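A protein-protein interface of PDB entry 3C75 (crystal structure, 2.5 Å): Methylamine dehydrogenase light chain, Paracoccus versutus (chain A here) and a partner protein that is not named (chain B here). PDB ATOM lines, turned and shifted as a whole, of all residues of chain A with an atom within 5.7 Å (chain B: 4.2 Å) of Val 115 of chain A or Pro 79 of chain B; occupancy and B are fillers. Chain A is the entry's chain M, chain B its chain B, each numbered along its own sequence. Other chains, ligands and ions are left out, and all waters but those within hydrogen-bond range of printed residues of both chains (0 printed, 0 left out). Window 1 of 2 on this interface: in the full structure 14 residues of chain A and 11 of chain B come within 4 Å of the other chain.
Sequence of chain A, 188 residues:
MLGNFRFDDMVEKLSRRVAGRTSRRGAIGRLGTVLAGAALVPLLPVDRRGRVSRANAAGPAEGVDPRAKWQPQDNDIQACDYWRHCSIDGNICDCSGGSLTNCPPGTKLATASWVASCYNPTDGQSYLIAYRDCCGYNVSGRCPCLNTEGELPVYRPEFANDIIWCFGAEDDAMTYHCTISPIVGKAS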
ATOM      1  N   SER A  87       0.678  23.900  21.408  1.00  0.00           N
ATOM      2  CA  SER A  87       1.074  23.035  20.303  1.00  0.00           C
ATOM      3  C   SER A  87       0.107  21.881  20.105  1.00  0.00           C
ATOM      4  O   SER A  87       0.490  20.759  19.792  1.00  0.00           O
ATOM      5  CB  SER A  87       2.491  22.505  20.503  1.00  0.00           C
ATOM      6  OG  SER A  87       3.086  22.290  19.237  1.00  0.00           O
ATOM      7  N   SER A 113       3.174  10.540  22.538  1.00  0.00           N
ATOM      8  CA  SER A 113       2.722  11.698  21.812  1.00  0.00           C
ATOM      9  C   SER A 113       3.780  12.737  21.533  1.00  0.00           C
ATOM     10  O   SER A 113       4.905  12.640  21.980  1.00  0.00           O
ATOM     11  CB  SER A 113       1.647  12.382  22.639  1.00  0.00           C
ATOM     12  OG  SER A 113       2.226  12.830  23.860  1.00  0.00           O
ATOM     13  N   TRQ A 114       3.373  13.766  20.809  1.00  0.00           N
ATOM     14  CA  TRQ A 114       4.252  14.877  20.518  1.00  0.00           C
ATOM     15  C   TRQ A 114       4.174  15.790  21.747  1.00  0.00           C
ATOM     16  O   TRQ A 114       3.143  15.867  22.420  1.00  0.00           O
ATOM     17  CB  TRQ A 114       3.802  15.588  19.231  1.00  0.00           C
ATOM     18  CG  TRQ A 114       2.495  16.326  19.314  1.00  0.00           C
ATOM     19  CD1 TRQ A 114       2.336  17.653  19.661  1.00  0.00           C
ATOM     20  NE1 TRQ A 114       1.017  18.011  19.583  1.00  0.00           N
ATOM     21  CE2 TRQ A 114       0.281  16.927  19.180  1.00  0.00           C
ATOM     22  CZ2 TRQ A 114      -1.094  16.826  18.962  1.00  0.00           C
ATOM     23  CH2 TRQ A 114      -1.609  15.588  18.548  1.00  0.00           C
ATOM     24  CZ3 TRQ A 114      -0.741  14.462  18.358  1.00  0.00           C
ATOM     25  CE3 TRQ A 114       0.642  14.575  18.584  1.00  0.00           C
ATOM     26  CD2 TRQ A 114       1.170  15.830  19.002  1.00  0.00           C
ATOM     27  O6  TRQ A 114      -2.875  15.449  18.387  1.00  0.00           O
ATOM     28  O7  TRQ A 114      -1.851  17.756  19.359  1.00  0.00           O
ATOM     29  N   VAL A 115       5.285  16.449  22.065  1.00  0.00           N
ATOM     30  CA  VAL A 115       5.323  17.323  23.235  1.00  0.00           C
ATOM     31  C   VAL A 115       5.652  18.727  22.797  1.00  0.00           C
ATOM     32  O   VAL A 115       5.819  18.992  21.614  1.00  0.00           O
ATOM     33  CB  VAL A 115       6.403  16.864  24.241  1.00  0.00           C
ATOM     34  CG1 VAL A 115       6.140  15.448  24.734  1.00  0.00           C
ATOM     35  CG2 VAL A 115       7.728  16.879  23.574  1.00  0.00           C
ATOM     36  N   ALA A 116       5.757  19.624  23.759  1.00  0.00           N
ATOM     37  CA  ALA A 116       6.093  21.008  23.471  1.00  0.00           C
ATOM     38  C   ALA A 116       6.239  21.797  24.739  1.00  0.00           C
ATOM     39  O   ALA A 116       5.442  21.690  25.665  1.00  0.00           O
ATOM     40  CB  ALA A 116       5.021  21.664  22.587  1.00  0.00           C
ATOM     41  N   SER A 117       7.285  22.597  24.779  1.00  0.00           N
ATOM     42  CA  SER A 117       7.517  23.444  25.930  1.00  0.00           C
ATOM     43  C   SER A 117       6.591  24.645  25.757  1.00  0.00           C
ATOM     44  O   SER A 117       6.638  25.338  24.724  1.00  0.00           O
ATOM     45  CB  SER A 117       8.947  23.916  25.970  1.00  0.00           C
ATOM     46  OG  SER A 117       8.973  25.079  26.765  1.00  0.00           O
ATOM     47  N   LEU A 128       6.640  21.057  29.887  1.00  0.00           N
ATOM     48  CA  LEU A 128       6.496  20.253  28.713  1.00  0.00           C
ATOM     49  C   LEU A 128       5.130  19.599  28.854  1.00  0.00           C
ATOM     50  O   LEU A 128       4.767  19.077  29.923  1.00  0.00           O
ATOM     51  CB  LEU A 128       7.594  19.209  28.672  1.00  0.00           C
ATOM     52  CG  LEU A 128       7.868  18.561  27.326  1.00  0.00           C
ATOM     53  CD1 LEU A 128       8.568  19.571  26.446  1.00  0.00           C
ATOM     54  CD2 LEU A 128       8.728  17.307  27.516  1.00  0.00           C
ATOM     55  N   ILE A 129       4.366  19.669  27.769  1.00  0.00           N
ATOM     56  CA  ILE A 129       3.026  19.105  27.728  1.00  0.00           C
ATOM     57  C   ILE A 129       3.108  17.909  26.801  1.00  0.00           C
ATOM     58  O   ILE A 129       3.775  17.990  25.759  1.00  0.00           O
ATOM     59  CB  ILE A 129       2.025  20.131  27.146  1.00  0.00           C
ATOM     60  CG1 ILE A 129       2.154  21.462  27.883  1.00  0.00           C
ATOM     61  CG2 ILE A 129       0.630  19.581  27.199  1.00  0.00           C
ATOM     62  CD1 ILE A 129       1.953  21.393  29.361  1.00  0.00           C
ATOM     63  N   ALA A 130       2.476  16.807  27.195  1.00  0.00           N
ATOM     64  CA  ALA A 130       2.461  15.607  26.374  1.00  0.00           C
ATOM     65  C   ALA A 130       1.081  15.579  25.752  1.00  0.00           C
ATOM     66  O   ALA A 130       0.101  15.218  26.418  1.00  0.00           O
ATOM     67  CB  ALA A 130       2.658  14.369  27.214  1.00  0.00           C
ATOM     68  N   TYR A 131       1.003  15.970  24.486  1.00  0.00           N
ATOM     69  CA  TYR A 131      -0.266  16.004  23.778  1.00  0.00           C
ATOM     70  C   TYR A 131      -0.705  14.622  23.329  1.00  0.00           C
ATOM     71  O   TYR A 131      -0.626  14.285  22.134  1.00  0.00           O
ATOM     72  CB  TYR A 131      -0.146  16.909  22.573  1.00  0.00           C
ATOM     73  CG  TYR A 131       0.087  18.357  22.930  1.00  0.00           C
ATOM     74  CD1 TYR A 131      -0.876  19.077  23.631  1.00  0.00           C
ATOM     75  CD2 TYR A 131       1.255  18.998  22.560  1.00  0.00           C
ATOM     76  CE1 TYR A 131      -0.679  20.413  23.950  1.00  0.00           C
ATOM     77  CE2 TYR A 131       1.483  20.334  22.882  1.00  0.00           C
ATOM     78  CZ  TYR A 131       0.514  21.054  23.576  1.00  0.00           C
ATOM     79  OH  TYR A 131       0.714  22.401  23.876  1.00  0.00           O
ATOM     80  N   GLU A 158       9.076  13.872  17.674  1.00  0.00           N
ATOM     81  CA  GLU A 158       8.815  14.324  19.039  1.00  0.00           C
ATOM     82  C   GLU A 158       8.137  15.688  19.125  1.00  0.00           C
ATOM     83  O   GLU A 158       7.492  15.998  20.137  1.00  0.00           O
ATOM     84  CB  GLU A 158      10.097  14.375  19.862  1.00  0.00           C
ATOM     85  CG  GLU A 158      11.235  13.565  19.303  1.00  0.00           C
ATOM     86  CD  GLU A 158      12.103  14.353  18.315  1.00  0.00           C
ATOM     87  OE1 GLU A 158      12.885  15.232  18.741  1.00  0.00           O
ATOM     88  OE2 GLU A 158      11.999  14.085  17.102  1.00  0.00           O
ATOM     89  N   PHE A 159       8.254  16.510  18.085  1.00  0.00           N
ATOM     90  CA  PHE A 159       7.618  17.847  18.121  1.00  0.00           C
ATOM     91  C   PHE A 159       6.690  18.102  16.942  1.00  0.00           C
ATOM     92  O   PHE A 159       6.251  19.240  16.712  1.00  0.00           O
ATOM     93  CB  PHE A 159       8.683  18.957  18.158  1.00  0.00           C
ATOM     94  CG  PHE A 159       9.565  18.909  19.372  1.00  0.00           C
ATOM     95  CD1 PHE A 159       9.117  19.396  20.598  1.00  0.00           C
ATOM     96  CD2 PHE A 159      10.845  18.360  19.295  1.00  0.00           C
ATOM     97  CE1 PHE A 159       9.947  19.331  21.746  1.00  0.00           C
ATOM     98  CE2 PHE A 159      11.684  18.288  20.433  1.00  0.00           C
ATOM     99  CZ  PHE A 159      11.238  18.770  21.656  1.00  0.00           C
ATOM    100  N   VAL A 184       4.028  17.038  31.677  1.00  0.00           N
ATOM    101  CA  VAL A 184       4.924  15.915  31.884  1.00  0.00           C
ATOM    102  C   VAL A 184       5.879  16.360  32.970  1.00  0.00           C
ATOM    103  O   VAL A 184       6.543  15.546  33.599  1.00  0.00           O
ATOM    104  CB  VAL A 184       5.725  15.568  30.613  1.00  0.00           C
ATOM    105  CG1 VAL A 184       4.801  15.168  29.523  1.00  0.00           C
ATOM    106  CG2 VAL A 184       6.488  16.740  30.156  1.00  0.00           C
ATOM    107  N   VAL B  77      13.380  15.395  30.466  1.00  0.00           N
ATOM    108  CA  VAL B  77      11.920  15.586  30.564  1.00  0.00           C
ATOM    109  C   VAL B  77      11.199  14.824  29.443  1.00  0.00           C
ATOM    110  O   VAL B  77      10.135  14.259  29.661  1.00  0.00           O
ATOM    111  CB  VAL B  77      11.487  17.110  30.438  1.00  0.00           C
ATOM    112  CG1 VAL B  77      11.038  17.658  31.787  1.00  0.00           C
ATOM    113  CG2 VAL B  77      12.628  17.936  29.881  1.00  0.00           C
ATOM    114  N   MET B  78      11.791  14.814  28.247  1.00  0.00           N
ATOM    115  CA  MET B  78      11.188  14.139  27.098  1.00  0.00           C
ATOM    116  C   MET B  78      10.741  12.750  27.513  1.00  0.00           C
ATOM    117  O   MET B  78      11.548  11.936  27.971  1.00  0.00           O
ATOM    118  CB  MET B  78      12.186  14.045  25.938  1.00  0.00           C
ATOM    119  CG  MET B  78      11.640  13.270  24.736  1.00  0.00           C
ATOM    120  SD  MET B  78      10.255  14.114  24.005  1.00  0.00           S
ATOM    121  CE  MET B  78      11.196  15.443  23.044  1.00  0.00           C
ATOM    122  N   PRO B  79       9.445  12.468  27.388  1.00  0.00           N
ATOM    123  CA  PRO B  79       8.972  11.146  27.781  1.00  0.00           C
ATOM    124  C   PRO B  79       9.542  10.082  26.872  1.00  0.00           C
ATOM    125  O   PRO B  79       9.638  10.271  25.674  1.00  0.00           O
ATOM    126  CB  PRO B  79       7.472  11.283  27.668  1.00  0.00           C
ATOM    127  CG  PRO B  79       7.255  12.777  27.965  1.00  0.00           C
ATOM    128  CD  PRO B  79       8.323  13.395  27.160  1.00  0.00           C
ATOM    129  N   HIS B  80       9.953   8.974  27.467  1.00  0.00           N
ATOM    130  CA  HIS B  80      10.528   7.856  26.722  1.00  0.00           C
ATOM    131  C   HIS B  80      10.160   6.541  27.402  1.00  0.00           C
ATOM    132  O   HIS B  80       9.783   6.512  28.572  1.00  0.00           O
ATOM    133  CB  HIS B  80      12.036   7.954  26.710  1.00  0.00           C
ATOM    134  CG  HIS B  80      12.585   9.132  25.970  1.00  0.00           C
ATOM    135  ND1 HIS B  80      12.443   9.290  24.609  1.00  0.00           N
ATOM    136  CD2 HIS B  80      13.399  10.135  26.378  1.00  0.00           C
ATOM    137  CE1 HIS B  80      13.156  10.327  24.208  1.00  0.00           C
ATOM    138  NE2 HIS B  80      13.746  10.856  25.262  1.00  0.00           N
ATOM    139  N   MET B  98       5.640   4.887  30.179  1.00  0.00           N
ATOM    140  CA  MET B  98       6.529   6.010  29.883  1.00  0.00           C
ATOM    141  C   MET B  98       7.270   6.462  31.124  1.00  0.00           C
ATOM    142  O   MET B  98       6.812   6.225  32.239  1.00  0.00           O
ATOM    143  CB  MET B  98       5.734   7.194  29.314  1.00  0.00           C
ATOM    144  CG  MET B  98       5.031   6.902  28.011  1.00  0.00           C
ATOM    145  SD  MET B  98       6.152   6.487  26.679  1.00  0.00           S
ATOM    146  CE  MET B  98       6.827   8.015  26.300  1.00  0.00           C
ATOM    147  N   MET B  99       8.417   7.099  30.899  1.00  0.00           N
ATOM    148  CA  MET B  99       9.273   7.666  31.949  1.00  0.00           C
ATOM    149  C   MET B  99       9.559   9.142  31.639  1.00  0.00           C
ATOM    150  O   MET B  99       9.831   9.493  30.484  1.00  0.00           O
ATOM    151  CB  MET B  99      10.646   6.972  31.993  1.00  0.00           C
ATOM    152  CG  MET B  99      10.667   5.522  32.402  1.00  0.00           C
ATOM    153  SD  MET B  99      12.307   4.868  32.310  1.00  0.00           S
ATOM    154  CE  MET B  99      12.325   4.257  30.596  1.00  0.00           C
ATOM    155  N   HIS B 122       8.958   7.355  19.632  1.00  0.00           N
ATOM    156  CA  HIS B 122      10.219   7.635  18.961  1.00  0.00           C
ATOM    157  C   HIS B 122      10.858   6.343  18.349  1.00  0.00           C
ATOM    158  O   HIS B 122      11.796   5.769  18.919  1.00  0.00           O
ATOM    159  CB  HIS B 122      11.144   8.307  19.991  1.00  0.00           C
ATOM    160  CG  HIS B 122      10.515   9.474  20.703  1.00  0.00           C
ATOM    161  ND1 HIS B 122      10.697   9.717  22.047  1.00  0.00           N
ATOM    162  CD2 HIS B 122       9.724  10.478  20.249  1.00  0.00           C
ATOM    163  CE1 HIS B 122      10.051  10.817  22.393  1.00  0.00           C
ATOM    164  NE2 HIS B 122       9.453  11.299  21.321  1.00  0.00           N
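The backbone NH (N) of Val 115 of chain A is in hydrogen-bond range of the backbone carbonyl oxygen (O) of Glu 158 of chain A, at 3.0 Å. The backbone NH (N) of Val 184 of chain A is in hydrogen-bond range of the backbone carbonyl oxygen (O) of Leu 128 of chain A.
CG2 of Val 115 of chain A touches SD of Met 78 of chain B (3.8 Å). Pro 79 of chain B touches Val 115 of chain A. Leu 128 of chain A touches Val 77 of chain B (CD2 to O, 3.98 Å). Leu 128 of chain A touches Pro 79 of chain B. CB of Glu 158 of chain A touches CE of Met 78 of chain B, 3.5 Å away. Glu 158 of chain A touches His 122 of chain B. CZ of Phe 159 of chain A touches CE of Met 78 of chain B (3.6 Å). CG1 of Val 184 of chain A touches CG of Pro 79 of chain B, 3.8 Å away.
Hydrophobic or aromatic side chains of chain B that line the printed part of chain A: Met 78, Pro 79 and His 122. Hydrophobic or aromatic side chains of chain A that line the printed part of chain B: Val 115, Leu 128, Phe 159 and Val 184. Among the printed residues, no Asp or Glu carboxylate lies within 4 Å of a Lys or Arg side-chain nitrogen of the other chain.
Val 115 of chain A touches two residues of chain B. Printed residues of chain A within 4 Å of Met 78 of chain B: Val 115, Glu 158 and Phe 159. Of the printed residues of chain A, Val 77 of chain B touches Leu 128 (3.98 Å). Of the printed residues of chain B, Leu 128 of chain A touches Val 77 and Pro 79. The nearest printed residue of chain B that does not touch Val 115 of chain A is His 122 of chain B (6.3 Å). The nearest printed residue of chain B that does not touch Glu 158 of chain A is His 80 of chain B (6.2 Å).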
